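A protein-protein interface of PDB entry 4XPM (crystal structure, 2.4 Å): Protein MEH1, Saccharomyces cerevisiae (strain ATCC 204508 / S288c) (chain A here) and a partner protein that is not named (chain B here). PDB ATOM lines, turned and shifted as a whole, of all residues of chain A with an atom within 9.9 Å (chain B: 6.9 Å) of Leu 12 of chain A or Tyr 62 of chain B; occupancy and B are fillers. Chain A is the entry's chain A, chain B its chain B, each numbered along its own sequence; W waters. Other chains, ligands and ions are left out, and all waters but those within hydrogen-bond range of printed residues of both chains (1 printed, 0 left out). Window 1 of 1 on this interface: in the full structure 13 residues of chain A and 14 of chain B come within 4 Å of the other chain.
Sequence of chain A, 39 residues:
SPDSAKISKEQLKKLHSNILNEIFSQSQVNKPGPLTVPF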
ATOM      1  N   SER A   1       7.443  10.012 -14.450  1.00  0.00           N
ATOM      2  CA  SER A   1       8.107   8.711 -14.338  1.00  0.00           C
ATOM      3  C   SER A   1       9.610   8.828 -14.047  1.00  0.00           C
ATOM      4  O   SER A   1      10.304   9.663 -14.629  1.00  0.00           O
ATOM      5  CB  SER A   1       7.880   7.874 -15.597  1.00  0.00           C
ATOM      6  OG  SER A   1       8.685   6.702 -15.593  1.00  0.00           O
ATOM      7  N   PRO A   2      10.119   7.976 -13.144  1.00  0.00           N
ATOM      8  CA  PRO A   2      11.529   8.037 -12.735  1.00  0.00           C
ATOM      9  C   PRO A   2      12.474   7.521 -13.811  1.00  0.00           C
ATOM     10  O   PRO A   2      12.082   6.703 -14.651  1.00  0.00           O
ATOM     11  CB  PRO A   2      11.591   7.100 -11.520  1.00  0.00           C
ATOM     12  CG  PRO A   2      10.156   6.845 -11.129  1.00  0.00           C
ATOM     13  CD  PRO A   2       9.371   6.952 -12.396  1.00  0.00           C
ATOM     14  N   ASP A   3      13.711   8.007 -13.786  1.00  0.00           N
ATOM     15  CA  ASP A   3      14.774   7.406 -14.577  1.00  0.00           C
ATOM     16  C   ASP A   3      15.536   6.468 -13.634  1.00  0.00           C
ATOM     17  O   ASP A   3      15.427   6.582 -12.412  1.00  0.00           O
ATOM     18  CB  ASP A   3      15.684   8.487 -15.180  1.00  0.00           C
ATOM     19  CG  ASP A   3      16.308   8.069 -16.521  1.00  0.00           C
ATOM     20  OD1 ASP A   3      16.528   6.860 -16.747  1.00  0.00           O
ATOM     21  OD2 ASP A   3      16.597   8.961 -17.349  1.00  0.00           O
ATOM     22  N   SER A   4      16.286   5.530 -14.203  1.00  0.00           N
ATOM     23  CA  SER A   4      16.984   4.510 -13.427  1.00  0.00           C
ATOM     24  C   SER A   4      18.375   4.292 -14.013  1.00  0.00           C
ATOM     25  O   SER A   4      18.566   4.414 -15.225  1.00  0.00           O
ATOM     26  CB  SER A   4      16.184   3.197 -13.437  1.00  0.00           C
ATOM     27  OG  SER A   4      16.949   2.097 -12.963  1.00  0.00           O
ATOM     28  N   LYS A   6      19.741   1.429 -13.803  1.00  0.00           N
ATOM     29  CA  LYS A   6      19.719   0.023 -14.206  1.00  0.00           C
ATOM     30  C   LYS A   6      19.523  -0.034 -15.713  1.00  0.00           C
ATOM     31  O   LYS A   6      20.222  -0.753 -16.411  1.00  0.00           O
ATOM     32  CB  LYS A   6      18.609  -0.760 -13.494  1.00  0.00           C
ATOM     33  CG  LYS A   6      18.483  -0.511 -11.996  1.00  0.00           C
ATOM     34  CD  LYS A   6      19.829  -0.442 -11.267  1.00  0.00           C
ATOM     35  CE  LYS A   6      20.528  -1.783 -11.162  1.00  0.00           C
ATOM     36  NZ  LYS A   6      21.778  -1.646 -10.359  1.00  0.00           N
ATOM     37  N   ILE A   7      18.553   0.727 -16.202  1.00  0.00           N
ATOM     38  CA  ILE A   7      18.436   1.018 -17.622  1.00  0.00           C
ATOM     39  C   ILE A   7      17.795   2.394 -17.756  1.00  0.00           C
ATOM     40  O   ILE A   7      16.712   2.629 -17.231  1.00  0.00           O
ATOM     41  CB  ILE A   7      17.635  -0.074 -18.394  1.00  0.00           C
ATOM     42  CG1 ILE A   7      17.512   0.299 -19.875  1.00  0.00           C
ATOM     43  CG2 ILE A   7      16.257  -0.318 -17.763  1.00  0.00           C
ATOM     44  CD1 ILE A   7      16.781  -0.733 -20.713  1.00  0.00           C
ATOM     45  N   SER A   8      18.469   3.315 -18.427  1.00  0.00           N
ATOM     46  CA  SER A   8      17.950   4.677 -18.524  1.00  0.00           C
ATOM     47  C   SER A   8      16.823   4.798 -19.545  1.00  0.00           C
ATOM     48  O   SER A   8      16.608   3.902 -20.350  1.00  0.00           O
ATOM     49  CB  SER A   8      19.070   5.672 -18.850  1.00  0.00           C
ATOM     50  OG  SER A   8      19.492   5.560 -20.193  1.00  0.00           O
ATOM     51  N   LYS A   9      16.103   5.911 -19.509  1.00  0.00           N
ATOM     52  CA  LYS A   9      15.017   6.137 -20.476  1.00  0.00           C
ATOM     53  C   LYS A   9      15.525   6.085 -21.923  1.00  0.00           C
ATOM     54  O   LYS A   9      14.906   5.453 -22.782  1.00  0.00           O
ATOM     55  CB  LYS A   9      14.312   7.470 -20.215  1.00  0.00           C
ATOM     56  CG  LYS A   9      13.300   7.435 -19.082  1.00  0.00           C
ATOM     57  CD  LYS A   9      12.839   8.843 -18.710  1.00  0.00           C
ATOM     58  CE  LYS A   9      11.913   8.819 -17.510  1.00  0.00           C
ATOM     59  NZ  LYS A   9      11.728  10.184 -16.942  1.00  0.00           N
ATOM     60  N   GLU A  10      16.651   6.758 -22.164  1.00  0.00           N
ATOM     61  CA  GLU A  10      17.318   6.787 -23.465  1.00  0.00           C
ATOM     62  C   GLU A  10      17.646   5.384 -23.954  1.00  0.00           C
ATOM     63  O   GLU A  10      17.336   5.029 -25.097  1.00  0.00           O
ATOM     64  CB  GLU A  10      18.598   7.637 -23.400  1.00  0.00           C
ATOM     65  CG  GLU A  10      18.371   9.148 -23.219  1.00  0.00           C
ATOM     66  CD  GLU A  10      17.908   9.532 -21.817  1.00  0.00           C
ATOM     67  OE1 GLU A  10      17.958   8.677 -20.898  1.00  0.00           O
ATOM     68  OE2 GLU A  10      17.494  10.699 -21.629  1.00  0.00           O
ATOM     69  N   GLN A  11      18.259   4.582 -23.085  1.00  0.00           N
ATOM     70  CA  GLN A  11      18.593   3.189 -23.434  1.00  0.00           C
ATOM     71  C   GLN A  11      17.350   2.359 -23.743  1.00  0.00           C
ATOM     72  O   GLN A  11      17.333   1.566 -24.683  1.00  0.00           O
ATOM     73  CB  GLN A  11      19.354   2.506 -22.294  1.00  0.00           C
ATOM     74  CG  GLN A  11      20.837   2.795 -22.254  1.00  0.00           C
ATOM     75  CD  GLN A  11      21.407   2.631 -20.852  1.00  0.00           C
ATOM     76  OE1 GLN A  11      20.733   2.919 -19.862  1.00  0.00           O
ATOM     77  NE2 GLN A  11      22.649   2.173 -20.765  1.00  0.00           N
ATOM     78  N   LEU A  12      16.324   2.539 -22.921  1.00  0.00           N
ATOM     79  CA  LEU A  12      15.102   1.769 -23.023  1.00  0.00           C
ATOM     80  C   LEU A  12      14.381   2.074 -24.341  1.00  0.00           C
ATOM     81  O   LEU A  12      13.983   1.162 -25.069  1.00  0.00           O
ATOM     82  CB  LEU A  12      14.211   2.077 -21.820  1.00  0.00           C
ATOM     83  CG  LEU A  12      12.811   1.483 -21.869  1.00  0.00           C
ATOM     84  CD1 LEU A  12      12.893  -0.024 -22.080  1.00  0.00           C
ATOM     85  CD2 LEU A  12      12.024   1.838 -20.603  1.00  0.00           C
ATOM     86  N   LYS A  13      14.233   3.364 -24.624  1.00  0.00           N
ATOM     87  CA  LYS A  13      13.687   3.859 -25.881  1.00  0.00           C
ATOM     88  C   LYS A  13      14.498   3.317 -27.068  1.00  0.00           C
ATOM     89  O   LYS A  13      13.945   2.792 -28.049  1.00  0.00           O
ATOM     90  CB  LYS A  13      13.744   5.387 -25.853  1.00  0.00           C
ATOM     91  CG  LYS A  13      13.013   6.106 -26.968  1.00  0.00           C
ATOM     92  CD  LYS A  13      12.836   7.577 -26.584  1.00  0.00           C
ATOM     93  CE  LYS A  13      12.362   8.419 -27.753  1.00  0.00           C
ATOM     94  NZ  LYS A  13      13.381   8.483 -28.841  1.00  0.00           N
ATOM     95  N   LYS A  14      15.817   3.420 -26.955  1.00  0.00           N
ATOM     96  CA  LYS A  14      16.711   2.943 -28.007  1.00  0.00           C
ATOM     97  C   LYS A  14      16.568   1.439 -28.253  1.00  0.00           C
ATOM     98  O   LYS A  14      16.571   0.980 -29.404  1.00  0.00           O
ATOM     99  CB  LYS A  14      18.164   3.333 -27.696  1.00  0.00           C
ATOM    100  CG  LYS A  14      19.208   2.871 -28.723  1.00  0.00           C
ATOM    101  CD  LYS A  14      18.895   3.349 -30.145  1.00  0.00           C
ATOM    102  CE  LYS A  14      20.087   3.068 -31.074  1.00  0.00           C
ATOM    103  NZ  LYS A  14      19.842   3.441 -32.495  1.00  0.00           N
ATOM    104  N   LEU A  15      16.429   0.675 -27.180  1.00  0.00           N
ATOM    105  CA  LEU A  15      16.217  -0.753 -27.316  1.00  0.00           C
ATOM    106  C   LEU A  15      14.853  -1.045 -27.968  1.00  0.00           C
ATOM    107  O   LEU A  15      14.698  -2.008 -28.713  1.00  0.00           O
ATOM    108  CB  LEU A  15      16.334  -1.429 -25.955  1.00  0.00           C
ATOM    109  CG  LEU A  15      15.985  -2.914 -25.915  1.00  0.00           C
ATOM    110  CD1 LEU A  15      16.922  -3.724 -26.796  1.00  0.00           C
ATOM    111  CD2 LEU A  15      16.022  -3.402 -24.480  1.00  0.00           C
ATOM    112  N   HIS A  16      13.865  -0.203 -27.691  1.00  0.00           N
ATOM    113  CA  HIS A  16      12.564  -0.354 -28.326  1.00  0.00           C
ATOM    114  C   HIS A  16      12.713  -0.126 -29.825  1.00  0.00           C
ATOM    115  O   HIS A  16      12.229  -0.918 -30.637  1.00  0.00           O
ATOM    116  CB  HIS A  16      11.577   0.636 -27.712  1.00  0.00           C
ATOM    117  CG  HIS A  16      10.212   0.615 -28.323  1.00  0.00           C
ATOM    118  ND1 HIS A  16       9.917   1.259 -29.504  1.00  0.00           N
ATOM    119  CD2 HIS A  16       9.044   0.072 -27.886  1.00  0.00           C
ATOM    120  CE1 HIS A  16       8.631   1.104 -29.776  1.00  0.00           C
ATOM    121  NE2 HIS A  16       8.079   0.388 -28.811  1.00  0.00           N
ATOM    122  N   SER A  17      13.410   0.940 -30.200  1.00  0.00           N
ATOM    123  CA  SER A  17      13.594   1.239 -31.624  1.00  0.00           C
ATOM    124  C   SER A  17      14.368   0.131 -32.355  1.00  0.00           C
ATOM    125  O   SER A  17      14.055  -0.187 -33.505  1.00  0.00           O
ATOM    126  CB  SER A  17      14.239   2.621 -31.835  1.00  0.00           C
ATOM    127  OG  SER A  17      15.529   2.524 -32.403  1.00  0.00           O
ATOM    128  N   ASN A  18      15.366  -0.458 -31.686  1.00  0.00           N
ATOM    129  CA  ASN A  18      16.159  -1.549 -32.270  1.00  0.00           C
ATOM    130  C   ASN A  18      15.320  -2.796 -32.549  1.00  0.00           C
ATOM    131  O   ASN A  18      15.367  -3.350 -33.650  1.00  0.00           O
ATOM    132  CB  ASN A  18      17.386  -1.887 -31.404  1.00  0.00           C
ATOM    133  CG  ASN A  18      18.422  -0.778 -31.420  1.00  0.00           C
ATOM    134  OD1 ASN A  18      18.374   0.123 -32.272  1.00  0.00           O
ATOM    135  ND2 ASN A  18      19.362  -0.825 -30.479  1.00  0.00           N
ATOM    136  N   ILE A  19      14.548  -3.230 -31.559  1.00  0.00           N
ATOM    137  CA  ILE A  19      13.649  -4.361 -31.753  1.00  0.00           C
ATOM    138  C   ILE A  19      12.697  -4.103 -32.941  1.00  0.00           C
ATOM    139  O   ILE A  19      12.546  -4.959 -33.818  1.00  0.00           O
ATOM    140  CB  ILE A  19      12.865  -4.665 -30.450  1.00  0.00           C
ATOM    141  CG1 ILE A  19      13.841  -4.993 -29.310  1.00  0.00           C
ATOM    142  CG2 ILE A  19      11.879  -5.819 -30.645  1.00  0.00           C
ATOM    143  CD1 ILE A  19      13.152  -5.189 -27.963  1.00  0.00           C
ATOM    144  N   LEU A  20      12.079  -2.918 -32.988  1.00  0.00           N
ATOM    145  CA  LEU A  20      11.152  -2.591 -34.079  1.00  0.00           C
ATOM    146  C   LEU A  20      11.868  -2.574 -35.423  1.00  0.00           C
ATOM    147  O   LEU A  20      11.403  -3.194 -36.386  1.00  0.00           O
ATOM    148  CB  LEU A  20      10.415  -1.255 -33.866  1.00  0.00           C
ATOM    149  CG  LEU A  20       9.474  -1.069 -32.668  1.00  0.00           C
ATOM    150  CD1 LEU A  20       8.273  -0.204 -33.037  1.00  0.00           C
ATOM    151  CD2 LEU A  20       9.039  -2.391 -32.028  1.00  0.00           C
ATOM    152  N   LEU B  44       0.896   5.272 -19.114  1.00  0.00           N
ATOM    153  CA  LEU B  44       2.262   5.768 -19.210  1.00  0.00           C
ATOM    154  C   LEU B  44       2.311   7.268 -19.033  1.00  0.00           C
ATOM    155  O   LEU B  44       1.279   7.932 -19.095  1.00  0.00           O
ATOM    156  CB  LEU B  44       2.878   5.366 -20.551  1.00  0.00           C
ATOM    157  CG  LEU B  44       2.686   3.865 -20.770  1.00  0.00           C
ATOM    158  CD1 LEU B  44       2.573   3.569 -22.229  1.00  0.00           C
ATOM    159  CD2 LEU B  44       3.820   3.069 -20.135  1.00  0.00           C
ATOM    160  N   ASP B  45       3.512   7.800 -18.800  1.00  0.00           N
ATOM    161  CA  ASP B  45       3.665   9.242 -18.674  1.00  0.00           C
ATOM    162  C   ASP B  45       3.547   9.901 -20.054  1.00  0.00           C
ATOM    163  O   ASP B  45       3.379   9.214 -21.068  1.00  0.00           O
ATOM    164  CB  ASP B  45       4.975   9.621 -17.947  1.00  0.00           C
ATOM    165  CG  ASP B  45       6.240   9.323 -18.768  1.00  0.00           C
ATOM    166  OD1 ASP B  45       6.150   9.008 -19.973  1.00  0.00           O
ATOM    167  OD2 ASP B  45       7.356   9.416 -18.196  1.00  0.00           O
ATOM    168  N   GLU B  47       5.619  10.970 -22.056  1.00  0.00           N
ATOM    169  CA  GLU B  47       6.612  10.546 -23.038  1.00  0.00           C
ATOM    170  C   GLU B  47       6.570   9.037 -23.325  1.00  0.00           C
ATOM    171  O   GLU B  47       7.362   8.534 -24.111  1.00  0.00           O
ATOM    172  CB  GLU B  47       8.012  10.973 -22.595  1.00  0.00           C
ATOM    173  CG  GLU B  47       8.177  12.486 -22.471  1.00  0.00           C
ATOM    174  CD  GLU B  47       9.459  12.885 -21.755  1.00  0.00           C
ATOM    175  OE1 GLU B  47      10.002  12.060 -20.983  1.00  0.00           O
ATOM    176  OE2 GLU B  47       9.928  14.027 -21.964  1.00  0.00           O
ATOM    177  N   GLY B  48       5.644   8.322 -22.693  1.00  0.00           N
ATOM    178  CA  GLY B  48       5.488   6.902 -22.941  1.00  0.00           C
ATOM    179  C   GLY B  48       6.203   5.976 -21.981  1.00  0.00           C
ATOM    180  O   GLY B  48       6.360   4.791 -22.284  1.00  0.00           O
ATOM    181  N   PHE B  49       6.633   6.494 -20.827  1.00  0.00           N
ATOM    182  CA  PHE B  49       7.388   5.683 -19.859  1.00  0.00           C
ATOM    183  C   PHE B  49       6.593   5.367 -18.588  1.00  0.00           C
ATOM    184  O   PHE B  49       5.731   6.146 -18.175  1.00  0.00           O
ATOM    185  CB  PHE B  49       8.692   6.380 -19.452  1.00  0.00           C
ATOM    186  CG  PHE B  49       9.714   6.528 -20.578  1.00  0.00           C
ATOM    187  CD1 PHE B  49      10.669   5.539 -20.815  1.00  0.00           C
ATOM    188  CD2 PHE B  49       9.750   7.680 -21.352  1.00  0.00           C
ATOM    189  CE1 PHE B  49      11.612   5.684 -21.818  1.00  0.00           C
ATOM    190  CE2 PHE B  49      10.701   7.829 -22.358  1.00  0.00           C
ATOM    191  CZ  PHE B  49      11.629   6.828 -22.592  1.00  0.00           C
ATOM    192  N   ALA B  50       6.894   4.223 -17.975  1.00  0.00           N
ATOM    193  CA  ALA B  50       6.395   3.891 -16.639  1.00  0.00           C
ATOM    194  C   ALA B  50       7.326   2.875 -15.964  1.00  0.00           C
ATOM    195  O   ALA B  50       8.128   2.213 -16.630  1.00  0.00           O
ATOM    196  CB  ALA B  50       4.942   3.337 -16.703  1.00  0.00           C
ATOM    197  N   HIS B  60      10.449  -1.958 -16.483  1.00  0.00           N
ATOM    198  CA  HIS B  60      10.553  -0.672 -17.139  1.00  0.00           C
ATOM    199  C   HIS B  60       9.727  -0.762 -18.413  1.00  0.00           C
ATOM    200  O   HIS B  60       9.947  -1.642 -19.259  1.00  0.00           O
ATOM    201  CB  HIS B  60      12.014  -0.364 -17.477  1.00  0.00           C
ATOM    202  CG  HIS B  60      12.940  -0.429 -16.299  1.00  0.00           C
ATOM    203  ND1 HIS B  60      13.387   0.699 -15.638  1.00  0.00           N
ATOM    204  CD2 HIS B  60      13.501  -1.484 -15.659  1.00  0.00           C
ATOM    205  CE1 HIS B  60      14.186   0.341 -14.648  1.00  0.00           C
ATOM    206  NE2 HIS B  60      14.270  -0.978 -14.636  1.00  0.00           N
ATOM    207  N   LEU B  61       8.753   0.128 -18.539  1.00  0.00           N
ATOM    208  CA  LEU B  61       7.870   0.132 -19.689  1.00  0.00           C
ATOM    209  C   LEU B  61       8.144   1.316 -20.594  1.00  0.00           C
ATOM    210  O   LEU B  61       8.310   2.440 -20.125  1.00  0.00           O
ATOM    211  CB  LEU B  61       6.413   0.204 -19.228  1.00  0.00           C
ATOM    212  CG  LEU B  61       5.888  -1.009 -18.468  1.00  0.00           C
ATOM    213  CD1 LEU B  61       4.500  -0.681 -17.914  1.00  0.00           C
ATOM    214  CD2 LEU B  61       5.832  -2.208 -19.401  1.00  0.00           C
ATOM    215  N   TYR B  62       8.194   1.058 -21.894  1.00  0.00           N
ATOM    216  CA  TYR B  62       8.148   2.131 -22.880  1.00  0.00           C
ATOM    217  C   TYR B  62       7.262   1.717 -24.043  1.00  0.00           C
ATOM    218  O   TYR B  62       7.356   0.594 -24.552  1.00  0.00           O
ATOM    219  CB  TYR B  62       9.546   2.505 -23.377  1.00  0.00           C
ATOM    220  CG  TYR B  62       9.548   3.544 -24.486  1.00  0.00           C
ATOM    221  CD1 TYR B  62       9.348   4.889 -24.205  1.00  0.00           C
ATOM    222  CD2 TYR B  62       9.728   3.172 -25.815  1.00  0.00           C
ATOM    223  CE1 TYR B  62       9.349   5.840 -25.215  1.00  0.00           C
ATOM    224  CE2 TYR B  62       9.728   4.116 -26.834  1.00  0.00           C
ATOM    225  CZ  TYR B  62       9.545   5.449 -26.531  1.00  0.00           C
ATOM    226  OH  TYR B  62       9.547   6.398 -27.541  1.00  0.00           O
ATOM    227  N   LYS B  63       6.401   2.634 -24.457  1.00  0.00           N
ATOM    228  CA  LYS B  63       5.469   2.342 -25.525  1.00  0.00           C
ATOM    229  C   LYS B  63       5.539   3.380 -26.617  1.00  0.00           C
ATOM    230  O   LYS B  63       5.428   4.579 -26.363  1.00  0.00           O
ATOM    231  CB  LYS B  63       4.048   2.276 -24.990  1.00  0.00           C
ATOM    232  CG  LYS B  63       3.008   1.843 -26.013  1.00  0.00           C
ATOM    233  CD  LYS B  63       1.602   2.009 -25.418  1.00  0.00           C
ATOM    234  CE  LYS B  63       0.531   1.355 -26.280  1.00  0.00           C
ATOM    235  NZ  LYS B  63      -0.793   1.804 -25.805  1.00  0.00           N
ATOM    236  N   ARG B  64       5.730   2.904 -27.837  1.00  0.00           N
ATOM    237  CA  ARG B  64       5.636   3.759 -29.001  1.00  0.00           C
ATOM    238  C   ARG B  64       5.163   2.919 -30.182  1.00  0.00           C
ATOM    239  O   ARG B  64       5.416   1.712 -30.231  1.00  0.00           O
ATOM    240  CB  ARG B  64       6.986   4.416 -29.301  1.00  0.00           C
ATOM    241  CG  ARG B  64       6.858   5.690 -30.103  1.00  0.00           C
ATOM    242  CD  ARG B  64       8.219   6.227 -30.489  1.00  0.00           C
ATOM    243  NE  ARG B  64       8.156   7.619 -30.915  1.00  0.00           N
ATOM    244  CZ  ARG B  64       8.256   8.022 -32.178  1.00  0.00           C
ATOM    245  NH1 ARG B  64       8.188   9.316 -32.469  1.00  0.00           N
ATOM    246  NH2 ARG B  64       8.432   7.134 -33.152  1.00  0.00           N
ATOM    247  N   ASN B  65       4.465   3.553 -31.120  1.00  0.00           N
ATOM    248  CA  ASN B  65       3.967   2.858 -32.307  1.00  0.00           C
ATOM    249  C   ASN B  65       3.166   1.608 -31.974  1.00  0.00           C
ATOM    250  O   ASN B  65       3.346   0.558 -32.596  1.00  0.00           O
ATOM    251  CB  ASN B  65       5.120   2.510 -33.245  1.00  0.00           C
ATOM    252  CG  ASN B  65       5.691   3.732 -33.932  1.00  0.00           C
ATOM    253  OD1 ASN B  65       6.854   4.077 -33.742  1.00  0.00           O
ATOM    254  ND2 ASN B  65       4.863   4.405 -34.729  1.00  0.00           N
ATOM    255  N   ILE B  67       3.404  -0.472 -29.771  1.00  0.00           N
ATOM    256  CA  ILE B  67       4.127  -1.577 -29.182  1.00  0.00           C
ATOM    257  C   ILE B  67       4.796  -1.211 -27.868  1.00  0.00           C
ATOM    258  O   ILE B  67       5.596  -0.260 -27.787  1.00  0.00           O
ATOM    259  CB  ILE B  67       5.177  -2.128 -30.140  1.00  0.00           C
ATOM    260  CG1 ILE B  67       4.477  -2.698 -31.378  1.00  0.00           C
ATOM    261  CG2 ILE B  67       6.060  -3.148 -29.405  1.00  0.00           C
ATOM    262  CD1 ILE B  67       5.409  -2.819 -32.609  1.00  0.00           C
ATOM    263  N   THR B  68       4.483  -1.992 -26.840  1.00  0.00           N
ATOM    264  CA  THR B  68       5.010  -1.732 -25.526  1.00  0.00           C
ATOM    265  C   THR B  68       6.210  -2.619 -25.291  1.00  0.00           C
ATOM    266  O   THR B  68       6.145  -3.812 -25.554  1.00  0.00           O
ATOM    267  CB  THR B  68       3.972  -2.028 -24.438  1.00  0.00           C
ATOM    268  OG1 THR B  68       2.803  -1.237 -24.667  1.00  0.00           O
ATOM    269  CG2 THR B  68       4.554  -1.707 -23.073  1.00  0.00           C
ATOM    270  N   LEU B  69       7.298  -2.032 -24.795  1.00  0.00           N
ATOM    271  CA  LEU B  69       8.472  -2.796 -24.394  1.00  0.00           C
ATOM    272  C   LEU B  69       8.566  -2.793 -22.869  1.00  0.00           C
ATOM    273  O   LEU B  69       8.481  -1.733 -22.223  1.00  0.00           O
ATOM    274  CB  LEU B  69       9.758  -2.210 -24.990  1.00  0.00           C
ATOM    275  CG  LEU B  69      11.085  -2.881 -24.550  1.00  0.00           C
ATOM    276  CD1 LEU B  69      11.140  -4.371 -24.949  1.00  0.00           C
ATOM    277  CD2 LEU B  69      12.305  -2.162 -25.086  1.00  0.00           C
ATOM    278  N   ALA B  70       8.721  -3.985 -22.301  1.00  0.00           N
ATOM    279  CA  ALA B  70       8.922  -4.145 -20.866  1.00  0.00           C
ATOM    280  C   ALA B  70      10.271  -4.803 -20.656  1.00  0.00           C
ATOM    281  O   ALA B  70      10.501  -5.890 -21.167  1.00  0.00           O
ATOM    282  CB  ALA B  70       7.849  -5.023 -20.292  1.00  0.00           C
ATOM    283  N   VAL B  71      11.177  -4.162 -19.930  1.00  0.00           N
ATOM    284  CA  VAL B  71      12.377  -4.879 -19.550  1.00  0.00           C
ATOM    285  C   VAL B  71      12.447  -5.048 -18.055  1.00  0.00           C
ATOM    286  O   VAL B  71      12.053  -4.163 -17.300  1.00  0.00           O
ATOM    287  CB  VAL B  71      13.704  -4.326 -20.177  1.00  0.00           C
ATOM    288  CG1 VAL B  71      13.424  -3.288 -21.241  1.00  0.00           C
ATOM    289  CG2 VAL B  71      14.666  -3.823 -19.127  1.00  0.00           C
HETATM  290  O   HOH W   1       9.651  10.576 -18.784  1.00  0.00           O
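Among the printed residues, merely in contact across the chains: Ser 1 of chain A with Asp 45 of chain B, Leu 12 of chain A with Val 71 of chain B, Lys 9 of chain A with Phe 49 of chain B, Lys 13 of chain A with Tyr 62 of chain B, His 16 of chain A with Leu 69 of chain B, His 16 of chain A with Tyr 62 of chain B, Ile 7 of chain A with His 60 of chain B, Ser 4 of chain A with His 60 of chain B, Leu 20 of chain A with Ile 67 of chain B, Ile 19 of chain A with Leu 69 of chain B, Leu 12 of chain A with Leu 69 of chain B, Leu 12 of chain A with Tyr 62 of chain B, Ser 1 of chain A with Ala 50 of chain B, Ser 1 of chain A with Phe 49 of chain B, Leu 12 of chain A with Leu 61 of chain B, Leu 12 of chain A with His 60 of chain B, Leu 15 of chain A with Leu 69 of chain B and Leu 12 of chain A with Phe 49 of chain B.
O of Arg 64 of chain B sits at hydrogen-bond distance from NE2 of His 16 of chain A (3.3 Å). O of Ile 67 of chain B lies within hydrogen-bond range of NE2 of His 16 of chain A (2.8 Å).
Of the printed residues of chain B, Ile 7 of chain A touches His 60 (3.6 Å). Leu 12 of chain A touches just these residues of chain B: Phe 49 (3.9 Å), His 60 (3.8 Å), Leu 61 (3.8 Å), Tyr 62 (3.7 Å), Leu 69 (3.7 Å) and Val 71 (3.4 Å). Printed residues of chain B within 4 Å of Lys 13 of chain A: Tyr 62 (3.5 Å). No residue of chain A comes within 4 Å of Gly 48 of chain B. Leu 61 of chain B touches just one residue of chain A: Leu 12. Tyr 62 of chain B touches just these residues of chain A: Leu 12, Lys 13 and His 16. Thr 68 of chain B touches none of the printed residues of chain A. The nearest residue of chain B that does not touch Leu 12 of chain A is Ala 50 of chain B (5.6 Å). The nearest printed residue of chain A that does not touch His 60 of chain B is Lys 6 of chain A (4.5 Å).
Water W1 lies within hydrogen-bond range of the side-chain carboxylate of Asp 45 of chain B, the side-chain carboxylate of Glu 47 of chain B and the side-chain amino group of Lys 9 of chain A.
The side-chain carboxylate of Asp 45 of chain B lies within hydrogen-bond range of the backbone NH of Gly 48 of chain B (2.9 Å). The backbone NH (N) of His 60 of chain B lies within hydrogen-bond range of the backbone carbonyl oxygen (O) of Val 71 of chain B, at 2.8 Å. O of Ala 50 of chain B lies within hydrogen-bond range of N of Leu 61 of chain B, at 2.9 Å. The side-chain carboxylate of Asp 45 of chain B lies within hydrogen-bond range of the backbone NH of Phe 49 of chain B (2.7 Å). The side-chain amino group (NZ) of Lys 9 of chain A is in hydrogen-bond range of the backbone carbonyl oxygen (O) of Ser 1 of chain A, at 2.8 Å. The side-chain carboxylate of Asp 3 of chain A is in hydrogen-bond range of the backbone NH of Lys 9 of chain A (3.0 Å).
Of the 19 printed residues of chain A, 10 touch a printed residue of chain B. Printed residues of chain A that touch a printed residue of chain B: Ser 1, Ser 4, Ile 7, Lys 9, Leu 12, Lys 13, Leu 15, His 16, Ile 19 and Leu 20. Hydrophobic or aromatic side chains of chain A within 4 Å of the printed part of chain B: Ile 7, Leu 12, Leu 15, His 16, Ile 19 and Leu 20. Printed residues of chain B that touch a printed residue of chain A: Asp 45, Phe 49, Ala 50, His 60, Leu 61, Tyr 62, Arg 64, Ile 67, Leu 69 and Val 71. Hydrophobic or aromatic side chains of chain B within 4 Å of the printed part of chain A: Phe 49, His 60, Tyr 62, Ile 67, Leu 69 and Val 71. Among the printed residues, no Asp or Glu carboxylate lies within 4 Å of a Lys or Arg side-chain nitrogen of the other chain.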
